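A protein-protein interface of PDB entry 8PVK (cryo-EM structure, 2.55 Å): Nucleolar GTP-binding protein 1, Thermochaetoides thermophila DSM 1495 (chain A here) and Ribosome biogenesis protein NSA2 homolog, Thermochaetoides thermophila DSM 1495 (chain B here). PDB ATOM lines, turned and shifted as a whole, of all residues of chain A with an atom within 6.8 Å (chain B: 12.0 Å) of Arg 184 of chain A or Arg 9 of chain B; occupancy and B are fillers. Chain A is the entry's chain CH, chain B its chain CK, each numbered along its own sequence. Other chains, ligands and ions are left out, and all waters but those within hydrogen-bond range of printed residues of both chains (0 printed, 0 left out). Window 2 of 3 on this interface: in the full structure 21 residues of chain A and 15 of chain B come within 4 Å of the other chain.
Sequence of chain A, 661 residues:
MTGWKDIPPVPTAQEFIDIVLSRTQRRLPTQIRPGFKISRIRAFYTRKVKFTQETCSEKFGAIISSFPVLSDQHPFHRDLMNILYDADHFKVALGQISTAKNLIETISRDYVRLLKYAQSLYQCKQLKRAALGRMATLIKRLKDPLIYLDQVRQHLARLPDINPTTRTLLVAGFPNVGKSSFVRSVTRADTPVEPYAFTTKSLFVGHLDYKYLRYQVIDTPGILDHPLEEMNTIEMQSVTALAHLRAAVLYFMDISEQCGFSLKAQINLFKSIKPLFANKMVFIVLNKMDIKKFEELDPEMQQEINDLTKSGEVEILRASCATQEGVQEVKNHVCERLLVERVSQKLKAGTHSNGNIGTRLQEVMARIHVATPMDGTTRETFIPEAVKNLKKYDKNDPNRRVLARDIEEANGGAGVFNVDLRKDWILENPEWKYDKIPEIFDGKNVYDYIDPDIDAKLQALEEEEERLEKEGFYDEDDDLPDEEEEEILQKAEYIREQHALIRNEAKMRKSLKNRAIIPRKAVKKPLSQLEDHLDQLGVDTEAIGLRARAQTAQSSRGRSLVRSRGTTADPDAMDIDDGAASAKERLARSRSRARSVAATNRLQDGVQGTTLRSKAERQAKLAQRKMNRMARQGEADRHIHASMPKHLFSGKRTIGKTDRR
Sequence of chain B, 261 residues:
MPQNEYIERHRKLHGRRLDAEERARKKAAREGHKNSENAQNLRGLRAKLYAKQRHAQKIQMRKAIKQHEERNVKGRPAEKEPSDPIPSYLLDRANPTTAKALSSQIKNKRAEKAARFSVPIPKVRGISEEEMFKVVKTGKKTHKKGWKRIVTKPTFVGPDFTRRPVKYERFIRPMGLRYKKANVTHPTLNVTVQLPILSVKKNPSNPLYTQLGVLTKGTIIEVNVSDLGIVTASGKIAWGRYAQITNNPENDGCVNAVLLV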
ATOM      1  N   LYS A 179      17.613  19.287   0.694  1.00  0.00           N
ATOM      2  CA  LYS A 179      16.571  19.357   1.716  1.00  0.00           C
ATOM      3  C   LYS A 179      16.850  18.395   2.865  1.00  0.00           C
ATOM      4  O   LYS A 179      16.796  18.780   4.041  1.00  0.00           O
ATOM      5  CB  LYS A 179      15.210  19.060   1.088  1.00  0.00           C
ATOM      6  CG  LYS A 179      14.868  19.943  -0.095  1.00  0.00           C
ATOM      7  CD  LYS A 179      13.445  19.711  -0.568  1.00  0.00           C
ATOM      8  CE  LYS A 179      13.220  18.267  -0.978  1.00  0.00           C
ATOM      9  NZ  LYS A 179      13.842  17.948  -2.292  1.00  0.00           N
ATOM     10  N   SER A 180      17.154  17.135   2.542  1.00  0.00           N
ATOM     11  CA  SER A 180      17.476  16.161   3.578  1.00  0.00           C
ATOM     12  C   SER A 180      18.772  16.509   4.294  1.00  0.00           C
ATOM     13  O   SER A 180      18.899  16.240   5.491  1.00  0.00           O
ATOM     14  CB  SER A 180      17.558  14.757   2.983  1.00  0.00           C
ATOM     15  OG  SER A 180      16.273  14.170   2.888  1.00  0.00           O
ATOM     16  N   SER A 181      19.734  17.110   3.589  1.00  0.00           N
ATOM     17  CA  SER A 181      20.962  17.558   4.240  1.00  0.00           C
ATOM     18  C   SER A 181      20.678  18.662   5.252  1.00  0.00           C
ATOM     19  O   SER A 181      21.230  18.655   6.358  1.00  0.00           O
ATOM     20  CB  SER A 181      21.968  18.036   3.195  1.00  0.00           C
ATOM     21  OG  SER A 181      22.459  16.949   2.431  1.00  0.00           O
ATOM     22  N   PHE A 182      19.802  19.606   4.896  1.00  0.00           N
ATOM     23  CA  PHE A 182      19.423  20.663   5.830  1.00  0.00           C
ATOM     24  C   PHE A 182      18.692  20.100   7.044  1.00  0.00           C
ATOM     25  O   PHE A 182      18.951  20.515   8.183  1.00  0.00           O
ATOM     26  CB  PHE A 182      18.559  21.705   5.122  1.00  0.00           C
ATOM     27  CG  PHE A 182      18.061  22.795   6.026  1.00  0.00           C
ATOM     28  CD1 PHE A 182      18.919  23.785   6.475  1.00  0.00           C
ATOM     29  CD2 PHE A 182      16.735  22.831   6.426  1.00  0.00           C
ATOM     30  CE1 PHE A 182      18.466  24.789   7.307  1.00  0.00           C
ATOM     31  CE2 PHE A 182      16.275  23.833   7.258  1.00  0.00           C
ATOM     32  CZ  PHE A 182      17.143  24.813   7.699  1.00  0.00           C
ATOM     33  N   VAL A 183      17.779  19.151   6.818  1.00  0.00           N
ATOM     34  CA  VAL A 183      17.023  18.565   7.923  1.00  0.00           C
ATOM     35  C   VAL A 183      17.937  17.744   8.832  1.00  0.00           C
ATOM     36  O   VAL A 183      17.803  17.782  10.061  1.00  0.00           O
ATOM     37  CB  VAL A 183      15.842  17.742   7.375  1.00  0.00           C
ATOM     38  CG1 VAL A 183      15.117  17.008   8.490  1.00  0.00           C
ATOM     39  CG2 VAL A 183      14.871  18.662   6.661  1.00  0.00           C
ATOM     40  N   ARG A 184      18.895  17.015   8.249  1.00  0.00           N
ATOM     41  CA  ARG A 184      19.887  16.303   9.051  1.00  0.00           C
ATOM     42  C   ARG A 184      20.776  17.261   9.831  1.00  0.00           C
ATOM     43  O   ARG A 184      21.209  16.934  10.942  1.00  0.00           O
ATOM     44  CB  ARG A 184      20.757  15.420   8.161  1.00  0.00           C
ATOM     45  CG  ARG A 184      20.110  14.137   7.695  1.00  0.00           C
ATOM     46  CD  ARG A 184      21.156  13.207   7.110  1.00  0.00           C
ATOM     47  NE  ARG A 184      21.835  12.430   8.138  1.00  0.00           N
ATOM     48  CZ  ARG A 184      21.484  11.203   8.499  1.00  0.00           C
ATOM     49  NH1 ARG A 184      20.463  10.581   7.931  1.00  0.00           N
ATOM     50  NH2 ARG A 184      22.174  10.584   9.453  1.00  0.00           N
ATOM     51  N   SER A 185      21.071  18.432   9.265  1.00  0.00           N
ATOM     52  CA  SER A 185      21.920  19.388   9.962  1.00  0.00           C
ATOM     53  C   SER A 185      21.196  20.025  11.143  1.00  0.00           C
ATOM     54  O   SER A 185      21.798  20.234  12.202  1.00  0.00           O
ATOM     55  CB  SER A 185      22.407  20.459   8.990  1.00  0.00           C
ATOM     56  OG  SER A 185      21.319  21.203   8.473  1.00  0.00           O
ATOM     57  N   VAL A 186      19.909  20.341  10.988  1.00  0.00           N
ATOM     58  CA  VAL A 186      19.207  21.074  12.039  1.00  0.00           C
ATOM     59  C   VAL A 186      18.493  20.179  13.053  1.00  0.00           C
ATOM     60  O   VAL A 186      18.289  20.611  14.198  1.00  0.00           O
ATOM     61  CB  VAL A 186      18.206  22.095  11.451  1.00  0.00           C
ATOM     62  CG1 VAL A 186      18.931  23.116  10.592  1.00  0.00           C
ATOM     63  CG2 VAL A 186      17.094  21.406  10.674  1.00  0.00           C
ATOM     64  N   THR A 187      18.114  18.960  12.683  1.00  0.00           N
ATOM     65  CA  THR A 187      17.357  18.081  13.565  1.00  0.00           C
ATOM     66  C   THR A 187      18.106  16.767  13.772  1.00  0.00           C
ATOM     67  O   THR A 187      19.216  16.569  13.274  1.00  0.00           O
ATOM     68  CB  THR A 187      15.953  17.810  13.008  1.00  0.00           C
ATOM     69  OG1 THR A 187      16.058  17.225  11.704  1.00  0.00           O
ATOM     70  CG2 THR A 187      15.147  19.095  12.921  1.00  0.00           C
ATOM     71  N   ARG A 188      17.476  15.868  14.525  1.00  0.00           N
ATOM     72  CA  ARG A 188      18.011  14.543  14.800  1.00  0.00           C
ATOM     73  C   ARG A 188      17.361  13.464  13.940  1.00  0.00           C
ATOM     74  O   ARG A 188      17.612  12.275  14.161  1.00  0.00           O
ATOM     75  CB  ARG A 188      17.837  14.206  16.284  1.00  0.00           C
ATOM     76  CG  ARG A 188      18.981  13.410  16.891  1.00  0.00           C
ATOM     77  CD  ARG A 188      18.738  13.131  18.366  1.00  0.00           C
ATOM     78  NE  ARG A 188      17.778  12.053  18.574  1.00  0.00           N
ATOM     79  CZ  ARG A 188      18.077  10.762  18.533  1.00  0.00           C
ATOM     80  NH1 ARG A 188      19.310  10.344  18.300  1.00  0.00           N
ATOM     81  NH2 ARG A 188      17.114   9.865  18.732  1.00  0.00           N
ATOM     82  N   ALA A 189      16.533  13.852  12.973  1.00  0.00           N
ATOM     83  CA  ALA A 189      15.827  12.886  12.144  1.00  0.00           C
ATOM     84  C   ALA A 189      16.789  12.146  11.224  1.00  0.00           C
ATOM     85  O   ALA A 189      17.738  12.727  10.690  1.00  0.00           O
ATOM     86  CB  ALA A 189      14.750  13.583  11.315  1.00  0.00           C
ATOM     87  N   ASP A 190      16.535  10.851  11.040  1.00  0.00           N
ATOM     88  CA  ASP A 190      17.384   9.994  10.218  1.00  0.00           C
ATOM     89  C   ASP A 190      16.757   9.878   8.830  1.00  0.00           C
ATOM     90  O   ASP A 190      16.131   8.879   8.476  1.00  0.00           O
ATOM     91  CB  ASP A 190      17.565   8.631  10.879  1.00  0.00           C
ATOM     92  CG  ASP A 190      18.536   7.741  10.128  1.00  0.00           C
ATOM     93  OD1 ASP A 190      19.345   8.266   9.334  1.00  0.00           O
ATOM     94  OD2 ASP A 190      18.489   6.510  10.332  1.00  0.00           O
ATOM     95  N   THR A 191      16.929  10.932   8.038  1.00  0.00           N
ATOM     96  CA  THR A 191      16.513  10.873   6.644  1.00  0.00           C
ATOM     97  C   THR A 191      17.733  10.702   5.747  1.00  0.00           C
ATOM     98  O   THR A 191      18.780  11.310   6.009  1.00  0.00           O
ATOM     99  CB  THR A 191      15.721  12.126   6.256  1.00  0.00           C
ATOM    100  OG1 THR A 191      15.358  12.068   4.870  1.00  0.00           O
ATOM    101  CG2 THR A 191      16.484  13.418   6.560  1.00  0.00           C
ATOM    102  N   PRO A 192      17.671   9.844   4.731  1.00  0.00           N
ATOM    103  CA  PRO A 192      18.869   9.565   3.932  1.00  0.00           C
ATOM    104  C   PRO A 192      19.232  10.710   3.000  1.00  0.00           C
ATOM    105  O   PRO A 192      18.370  11.424   2.482  1.00  0.00           O
ATOM    106  CB  PRO A 192      18.480   8.310   3.137  1.00  0.00           C
ATOM    107  CG  PRO A 192      17.318   7.723   3.883  1.00  0.00           C
ATOM    108  CD  PRO A 192      16.584   8.897   4.443  1.00  0.00           C
ATOM    109  N   VAL A 193      20.536  10.871   2.784  1.00  0.00           N
ATOM    110  CA  VAL A 193      21.079  11.849   1.846  1.00  0.00           C
ATOM    111  C   VAL A 193      21.877  11.084   0.799  1.00  0.00           C
ATOM    112  O   VAL A 193      22.900  10.466   1.119  1.00  0.00           O
ATOM    113  CB  VAL A 193      21.954  12.897   2.550  1.00  0.00           C
ATOM    114  CG1 VAL A 193      22.774  13.685   1.538  1.00  0.00           C
ATOM    115  CG2 VAL A 193      21.101  13.826   3.388  1.00  0.00           C
ATOM    116  N   GLU A 194      21.394  11.100  -0.441  1.00  0.00           N
ATOM    117  CA  GLU A 194      22.005  10.403  -1.564  1.00  0.00           C
ATOM    118  C   GLU A 194      21.935  11.295  -2.796  1.00  0.00           C
ATOM    119  O   GLU A 194      21.046  12.150  -2.890  1.00  0.00           O
ATOM    120  CB  GLU A 194      21.308   9.059  -1.848  1.00  0.00           C
ATOM    121  CG  GLU A 194      21.070   8.148  -0.651  1.00  0.00           C
ATOM    122  CD  GLU A 194      22.293   7.332  -0.289  1.00  0.00           C
ATOM    123  OE1 GLU A 194      22.472   7.028   0.909  1.00  0.00           O
ATOM    124  OE2 GLU A 194      23.076   6.995  -1.202  1.00  0.00           O
ATOM    125  N   PHE A 204       9.215  13.036   6.241  1.00  0.00           N
ATOM    126  CA  PHE A 204      10.018  12.839   7.438  1.00  0.00           C
ATOM    127  C   PHE A 204       9.846  14.047   8.346  1.00  0.00           C
ATOM    128  O   PHE A 204       9.582  15.155   7.877  1.00  0.00           O
ATOM    129  CB  PHE A 204      11.501  12.656   7.100  1.00  0.00           C
ATOM    130  CG  PHE A 204      11.841  11.305   6.540  1.00  0.00           C
ATOM    131  CD1 PHE A 204      11.592  11.007   5.211  1.00  0.00           C
ATOM    132  CD2 PHE A 204      12.425  10.338   7.341  1.00  0.00           C
ATOM    133  CE1 PHE A 204      11.913   9.767   4.693  1.00  0.00           C
ATOM    134  CE2 PHE A 204      12.748   9.095   6.829  1.00  0.00           C
ATOM    135  CZ  PHE A 204      12.492   8.811   5.503  1.00  0.00           C
ATOM    136  N   ASP A 219      10.688  17.305   6.345  1.00  0.00           N
ATOM    137  CA  ASP A 219      11.378  17.008   5.100  1.00  0.00           C
ATOM    138  C   ASP A 219      10.410  16.317   4.151  1.00  0.00           C
ATOM    139  O   ASP A 219       9.700  15.382   4.544  1.00  0.00           O
ATOM    140  CB  ASP A 219      12.591  16.116   5.360  1.00  0.00           C
ATOM    141  CG  ASP A 219      13.404  15.848   4.110  1.00  0.00           C
ATOM    142  OD1 ASP A 219      13.313  16.643   3.151  1.00  0.00           O
ATOM    143  OD2 ASP A 219      14.139  14.840   4.087  1.00  0.00           O
ATOM    144  N   GLN A 324      28.217  23.561   6.325  1.00  0.00           N
ATOM    145  CA  GLN A 324      27.444  24.063   7.467  1.00  0.00           C
ATOM    146  C   GLN A 324      27.596  25.572   7.650  1.00  0.00           C
ATOM    147  O   GLN A 324      27.627  26.070   8.777  1.00  0.00           O
ATOM    148  CB  GLN A 324      27.807  23.327   8.761  1.00  0.00           C
ATOM    149  CG  GLN A 324      27.547  21.832   8.720  1.00  0.00           C
ATOM    150  CD  GLN A 324      26.078  21.507   8.559  1.00  0.00           C
ATOM    151  OE1 GLN A 324      25.221  22.157   9.158  1.00  0.00           O
ATOM    152  NE2 GLN A 324      25.778  20.496   7.753  1.00  0.00           N
ATOM    153  N   PRO B   2      10.725   6.156  15.504  1.00  0.00           N
ATOM    154  CA  PRO B   2      11.185   5.868  14.148  1.00  0.00           C
ATOM    155  C   PRO B   2      10.062   6.060  13.142  1.00  0.00           C
ATOM    156  O   PRO B   2       8.887   6.006  13.505  1.00  0.00           O
ATOM    157  CB  PRO B   2      11.616   4.410  14.235  1.00  0.00           C
ATOM    158  CG  PRO B   2      10.698   3.837  15.228  1.00  0.00           C
ATOM    159  CD  PRO B   2      10.397   4.922  16.232  1.00  0.00           C
ATOM    160  N   GLN B   3      10.422   6.289  11.884  1.00  0.00           N
ATOM    161  CA  GLN B   3       9.445   6.613  10.859  1.00  0.00           C
ATOM    162  C   GLN B   3       9.801   5.888   9.572  1.00  0.00           C
ATOM    163  O   GLN B   3      10.976   5.633   9.292  1.00  0.00           O
ATOM    164  CB  GLN B   3       9.382   8.127  10.630  1.00  0.00           C
ATOM    165  CG  GLN B   3      10.749   8.787  10.583  1.00  0.00           C
ATOM    166  CD  GLN B   3      10.685  10.283  10.805  1.00  0.00           C
ATOM    167  OE1 GLN B   3       9.609  10.874  10.817  1.00  0.00           O
ATOM    168  NE2 GLN B   3      11.843  10.903  10.988  1.00  0.00           N
ATOM    169  N   ASN B   4       8.765   5.547   8.811  1.00  0.00           N
ATOM    170  CA  ASN B   4       8.841   4.943   7.466  1.00  0.00           C
ATOM    171  C   ASN B   4       9.522   3.574   7.593  1.00  0.00           C
ATOM    172  O   ASN B   4       9.254   2.842   8.556  1.00  0.00           O
ATOM    173  CB  ASN B   4       9.491   5.919   6.509  1.00  0.00           C
ATOM    174  CG  ASN B   4       8.770   7.251   6.471  1.00  0.00           C
ATOM    175  OD1 ASN B   4       7.559   7.304   6.263  1.00  0.00           O
ATOM    176  ND2 ASN B   4       9.503   8.332   6.691  1.00  0.00           N
ATOM    177  N   GLU B   5      10.385   3.191   6.653  1.00  0.00           N
ATOM    178  CA  GLU B   5      10.951   1.840   6.628  1.00  0.00           C
ATOM    179  C   GLU B   5      12.234   1.787   7.460  1.00  0.00           C
ATOM    180  O   GLU B   5      13.347   1.598   6.960  1.00  0.00           O
ATOM    181  CB  GLU B   5      11.192   1.398   5.191  1.00  0.00           C
ATOM    182  CG  GLU B   5       9.978   0.775   4.526  1.00  0.00           C
ATOM    183  CD  GLU B   5       8.952   1.801   4.097  1.00  0.00           C
ATOM    184  OE1 GLU B   5       7.870   1.860   4.719  1.00  0.00           O
ATOM    185  OE2 GLU B   5       9.224   2.549   3.134  1.00  0.00           O
ATOM    186  N   TYR B   6      12.050   1.930   8.776  1.00  0.00           N
ATOM    187  CA  TYR B   6      13.200   2.036   9.665  1.00  0.00           C
ATOM    188  C   TYR B   6      13.901   0.701   9.883  1.00  0.00           C
ATOM    189  O   TYR B   6      15.118   0.681  10.076  1.00  0.00           O
ATOM    190  CB  TYR B   6      12.790   2.656  11.005  1.00  0.00           C
ATOM    191  CG  TYR B   6      11.607   2.019  11.702  1.00  0.00           C
ATOM    192  CD1 TYR B   6      11.783   0.955  12.579  1.00  0.00           C
ATOM    193  CD2 TYR B   6      10.322   2.512  11.521  1.00  0.00           C
ATOM    194  CE1 TYR B   6      10.711   0.384  13.231  1.00  0.00           C
ATOM    195  CE2 TYR B   6       9.244   1.949  12.172  1.00  0.00           C
ATOM    196  CZ  TYR B   6       9.444   0.884  13.025  1.00  0.00           C
ATOM    197  OH  TYR B   6       8.372   0.318  13.673  1.00  0.00           O
ATOM    198  N   ILE B   7      13.175  -0.419   9.835  1.00  0.00           N
ATOM    199  CA  ILE B   7      13.828  -1.721   9.962  1.00  0.00           C
ATOM    200  C   ILE B   7      14.656  -2.029   8.716  1.00  0.00           C
ATOM    201  O   ILE B   7      15.770  -2.562   8.811  1.00  0.00           O
ATOM    202  CB  ILE B   7      12.783  -2.814  10.261  1.00  0.00           C
ATOM    203  CG1 ILE B   7      12.279  -2.679  11.701  1.00  0.00           C
ATOM    204  CG2 ILE B   7      13.345  -4.213  10.040  1.00  0.00           C
ATOM    205  CD1 ILE B   7      13.335  -2.938  12.750  1.00  0.00           C
ATOM    206  N   GLU B   8      14.144  -1.672   7.534  1.00  0.00           N
ATOM    207  CA  GLU B   8      14.933  -1.808   6.311  1.00  0.00           C
ATOM    208  C   GLU B   8      16.158  -0.899   6.334  1.00  0.00           C
ATOM    209  O   GLU B   8      17.241  -1.292   5.880  1.00  0.00           O
ATOM    210  CB  GLU B   8      14.071  -1.507   5.086  1.00  0.00           C
ATOM    211  CG  GLU B   8      13.021  -2.560   4.787  1.00  0.00           C
ATOM    212  CD  GLU B   8      11.994  -2.085   3.778  1.00  0.00           C
ATOM    213  OE1 GLU B   8      12.295  -1.134   3.026  1.00  0.00           O
ATOM    214  OE2 GLU B   8      10.886  -2.658   3.738  1.00  0.00           O
ATOM    215  N   ARG B   9      16.007   0.319   6.864  1.00  0.00           N
ATOM    216  CA  ARG B   9      17.156   1.211   6.997  1.00  0.00           C
ATOM    217  C   ARG B   9      18.183   0.655   7.978  1.00  0.00           C
ATOM    218  O   ARG B   9      19.394   0.771   7.750  1.00  0.00           O
ATOM    219  CB  ARG B   9      16.692   2.604   7.424  1.00  0.00           C
ATOM    220  CG  ARG B   9      17.822   3.600   7.608  1.00  0.00           C
ATOM    221  CD  ARG B   9      17.471   4.959   7.036  1.00  0.00           C
ATOM    222  NE  ARG B   9      18.582   5.894   7.156  1.00  0.00           N
ATOM    223  CZ  ARG B   9      19.582   5.984   6.290  1.00  0.00           C
ATOM    224  NH1 ARG B   9      19.642   5.212   5.219  1.00  0.00           N
ATOM    225  NH2 ARG B   9      20.548   6.874   6.505  1.00  0.00           N
ATOM    226  N   HIS B  10      17.719   0.045   9.072  1.00  0.00           N
ATOM    227  CA  HIS B  10      18.624  -0.589  10.025  1.00  0.00           C
ATOM    228  C   HIS B  10      19.355  -1.769   9.398  1.00  0.00           C
ATOM    229  O   HIS B  10      20.538  -1.991   9.672  1.00  0.00           O
ATOM    230  CB  HIS B  10      17.851  -1.038  11.263  1.00  0.00           C
ATOM    231  CG  HIS B  10      18.724  -1.545  12.368  1.00  0.00           C
ATOM    232  ND1 HIS B  10      19.280  -0.715  13.317  1.00  0.00           N
ATOM    233  CD2 HIS B  10      19.138  -2.797  12.675  1.00  0.00           C
ATOM    234  CE1 HIS B  10      20.000  -1.433  14.161  1.00  0.00           C
ATOM    235  NE2 HIS B  10      19.930  -2.699  13.793  1.00  0.00           N
ATOM    236  N   ARG B  11      18.659  -2.545   8.563  1.00  0.00           N
ATOM    237  CA  ARG B  11      19.308  -3.653   7.869  1.00  0.00           C
ATOM    238  C   ARG B  11      20.338  -3.152   6.866  1.00  0.00           C
ATOM    239  O   ARG B  11      21.372  -3.796   6.656  1.00  0.00           O
ATOM    240  CB  ARG B  11      18.265  -4.524   7.171  1.00  0.00           C
ATOM    241  CG  ARG B  11      18.760  -5.920   6.834  1.00  0.00           C
ATOM    242  CD  ARG B  11      17.825  -6.627   5.866  1.00  0.00           C
ATOM    243  NE  ARG B  11      16.423  -6.447   6.222  1.00  0.00           N
ATOM    244  CZ  ARG B  11      15.513  -5.905   5.425  1.00  0.00           C
ATOM    245  NH1 ARG B  11      15.824  -5.476   4.212  1.00  0.00           N
ATOM    246  NH2 ARG B  11      14.259  -5.789   5.854  1.00  0.00           N
ATOM    247  N   LYS B  12      20.064  -2.018   6.222  1.00  0.00           N
ATOM    248  CA  LYS B  12      21.053  -1.427   5.323  1.00  0.00           C
ATOM    249  C   LYS B  12      22.271  -0.919   6.088  1.00  0.00           C
ATOM    250  O   LYS B  12      23.411  -1.135   5.664  1.00  0.00           O
ATOM    251  CB  LYS B  12      20.416  -0.294   4.521  1.00  0.00           C
ATOM    252  CG  LYS B  12      21.348   0.353   3.512  1.00  0.00           C
ATOM    253  CD  LYS B  12      20.620   1.391   2.674  1.00  0.00           C
ATOM    254  CE  LYS B  12      21.580   2.143   1.770  1.00  0.00           C
ATOM    255  NZ  LYS B  12      22.180   1.255   0.737  1.00  0.00           N
ATOM    256  N   LEU B  13      22.050  -0.247   7.220  1.00  0.00           N
ATOM    257  CA  LEU B  13      23.144   0.407   7.931  1.00  0.00           C
ATOM    258  C   LEU B  13      23.993  -0.575   8.733  1.00  0.00           C
ATOM    259  O   LEU B  13      25.217  -0.424   8.796  1.00  0.00           O
ATOM    260  CB  LEU B  13      22.590   1.494   8.852  1.00  0.00           C
ATOM    261  CG  LEU B  13      22.083   2.764   8.167  1.00  0.00           C
ATOM    262  CD1 LEU B  13      21.440   3.696   9.180  1.00  0.00           C
ATOM    263  CD2 LEU B  13      23.212   3.461   7.431  1.00  0.00           C
ATOM    264  N   HIS B  14      23.372  -1.577   9.355  1.00  0.00           N
ATOM    265  CA  HIS B  14      24.066  -2.446  10.294  1.00  0.00           C
ATOM    266  C   HIS B  14      24.017  -3.923   9.938  1.00  0.00           C
ATOM    267  O   HIS B  14      24.684  -4.719  10.608  1.00  0.00           O
ATOM    268  CB  HIS B  14      23.493  -2.268  11.709  1.00  0.00           C
ATOM    269  CG  HIS B  14      23.362  -0.841  12.135  1.00  0.00           C
ATOM    270  ND1 HIS B  14      22.179  -0.141  12.042  1.00  0.00           N
ATOM    271  CD2 HIS B  14      24.268   0.021  12.657  1.00  0.00           C
ATOM    272  CE1 HIS B  14      22.360   1.088  12.487  1.00  0.00           C
ATOM    273  NE2 HIS B  14      23.619   1.213  12.865  1.00  0.00           N
ATOM    274  N   GLY B  15      23.256  -4.317   8.923  1.00  0.00           N
ATOM    275  CA  GLY B  15      23.141  -5.721   8.590  1.00  0.00           C
ATOM    276  C   GLY B  15      22.228  -6.465   9.549  1.00  0.00           C
ATOM    277  O   GLY B  15      21.362  -5.891  10.217  1.00  0.00           O
ATOM    278  N   ARG B  16      22.437  -7.774   9.611  1.00  0.00           N
ATOM    279  CA  ARG B  16      21.682  -8.659  10.486  1.00  0.00           C
ATOM    280  C   ARG B  16      22.634  -9.318  11.483  1.00  0.00           C
ATOM    281  O   ARG B  16      23.816  -8.973  11.566  1.00  0.00           O
ATOM    282  CB  ARG B  16      20.919  -9.699   9.664  1.00  0.00           C
ATOM    283  CG  ARG B  16      19.817  -9.119   8.799  1.00  0.00           C
ATOM    284  CD  ARG B  16      19.121 -10.203   7.998  1.00  0.00           C
ATOM    285  NE  ARG B  16      19.996 -10.791   6.992  1.00  0.00           N
ATOM    286  CZ  ARG B  16      19.680 -11.846   6.252  1.00  0.00           C
ATOM    287  NH1 ARG B  16      18.519 -12.463   6.387  1.00  0.00           N
ATOM    288  NH2 ARG B  16      20.554 -12.293   5.354  1.00  0.00           N
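OD2 of Asp 190 of chain A lies within salt-bridge range of NE of Arg 9 of chain B.
Arg 9 of chain B touches three residues of chain A.
No residue of chain B comes within 4 Å of Ser 180 of chain A.
No residue of chain B comes within 4 Å of Ser 181 of chain A.
No residue of chain B comes within 4 Å of Val 183 of chain A.
No residue of chain B comes within 4 Å of Val 186 of chain A.
No residue of chain B comes within 4 Å of Thr 187 of chain A.
Of chain B, only Gln 3 (3.97 Å) comes within 4 Å of Ala 189 of chain A.
Of chain B, only Arg 9 (3.2 Å) comes within 4 Å of Asp 190 of chain A.
No residue of chain B comes within 4 Å of Thr 191 of chain A.
Of chain B, only Arg 9 (3.7 Å) comes within 4 Å of Pro 192 of chain A.
Of the printed residues of chain A, Gln 3 of chain B touches Ala 189 (3.97 Å) and Phe 204 (3.7 Å).
Of the printed residues of chain A, Asn 4 of chain B touches Phe 204 (3.3 Å).
Printed residues of chain B within 4 Å of Phe 204 of chain A: Gln 3 (3.7 Å) and Asn 4 (3.3 Å).
The nearest residue of chain A that does not touch Arg 9 of chain B is Thr 191 of chain A (4.8 Å).
The nearest printed residue of chain A that does not touch Gln 3 of chain B is Asp 190 of chain A (4.7 Å).
NH1 of Arg 184 of chain A touches NH2 of Arg 9 of chain B, 3.97 Å away.
Ala 189 of chain A touches Gln 3 of chain B (CB to NE2, 3.97 Å).
Pro 192 of chain A touches Arg 9 of chain B (CG to NH1, 3.7 Å).
NE2 of Gln 3 of chain B touches CD2 of Phe 204 of chain A, at 3.7 Å.
Asn 4 of chain B touches Phe 204 of chain A.
Of the 15 printed residues of chain B, 3 touch a printed residue of chain A.
Printed residues of chain A that touch a printed residue of chain B: Arg 184, Ala 189, Asp 190, Pro 192 and Phe 204.
Hydrophobic or aromatic side chains of chain A within 4 Å of the printed part of chain B: Ala 189, Pro 192 and Phe 204.
The backbone carbonyl oxygen (O) of Pro 192 of chain A sits close to the side-chain hydroxyl (OG) of Ser 180 of chain A (3.5 Å).
NH1 of Arg 184 of chain A is in salt-bridge range of OD1 of Asp 190 of chain A.
The guanidinium group of Arg 184 of chain A is in hydrogen-bond range of the backbone carbonyl oxygen of Thr 191 of chain A, 2.7 Å away.
The backbone NH (N) of Asp 219 of chain A lies within hydrogen-bond range of the backbone carbonyl oxygen (O) of Phe 204 of chain A (2.9 Å).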
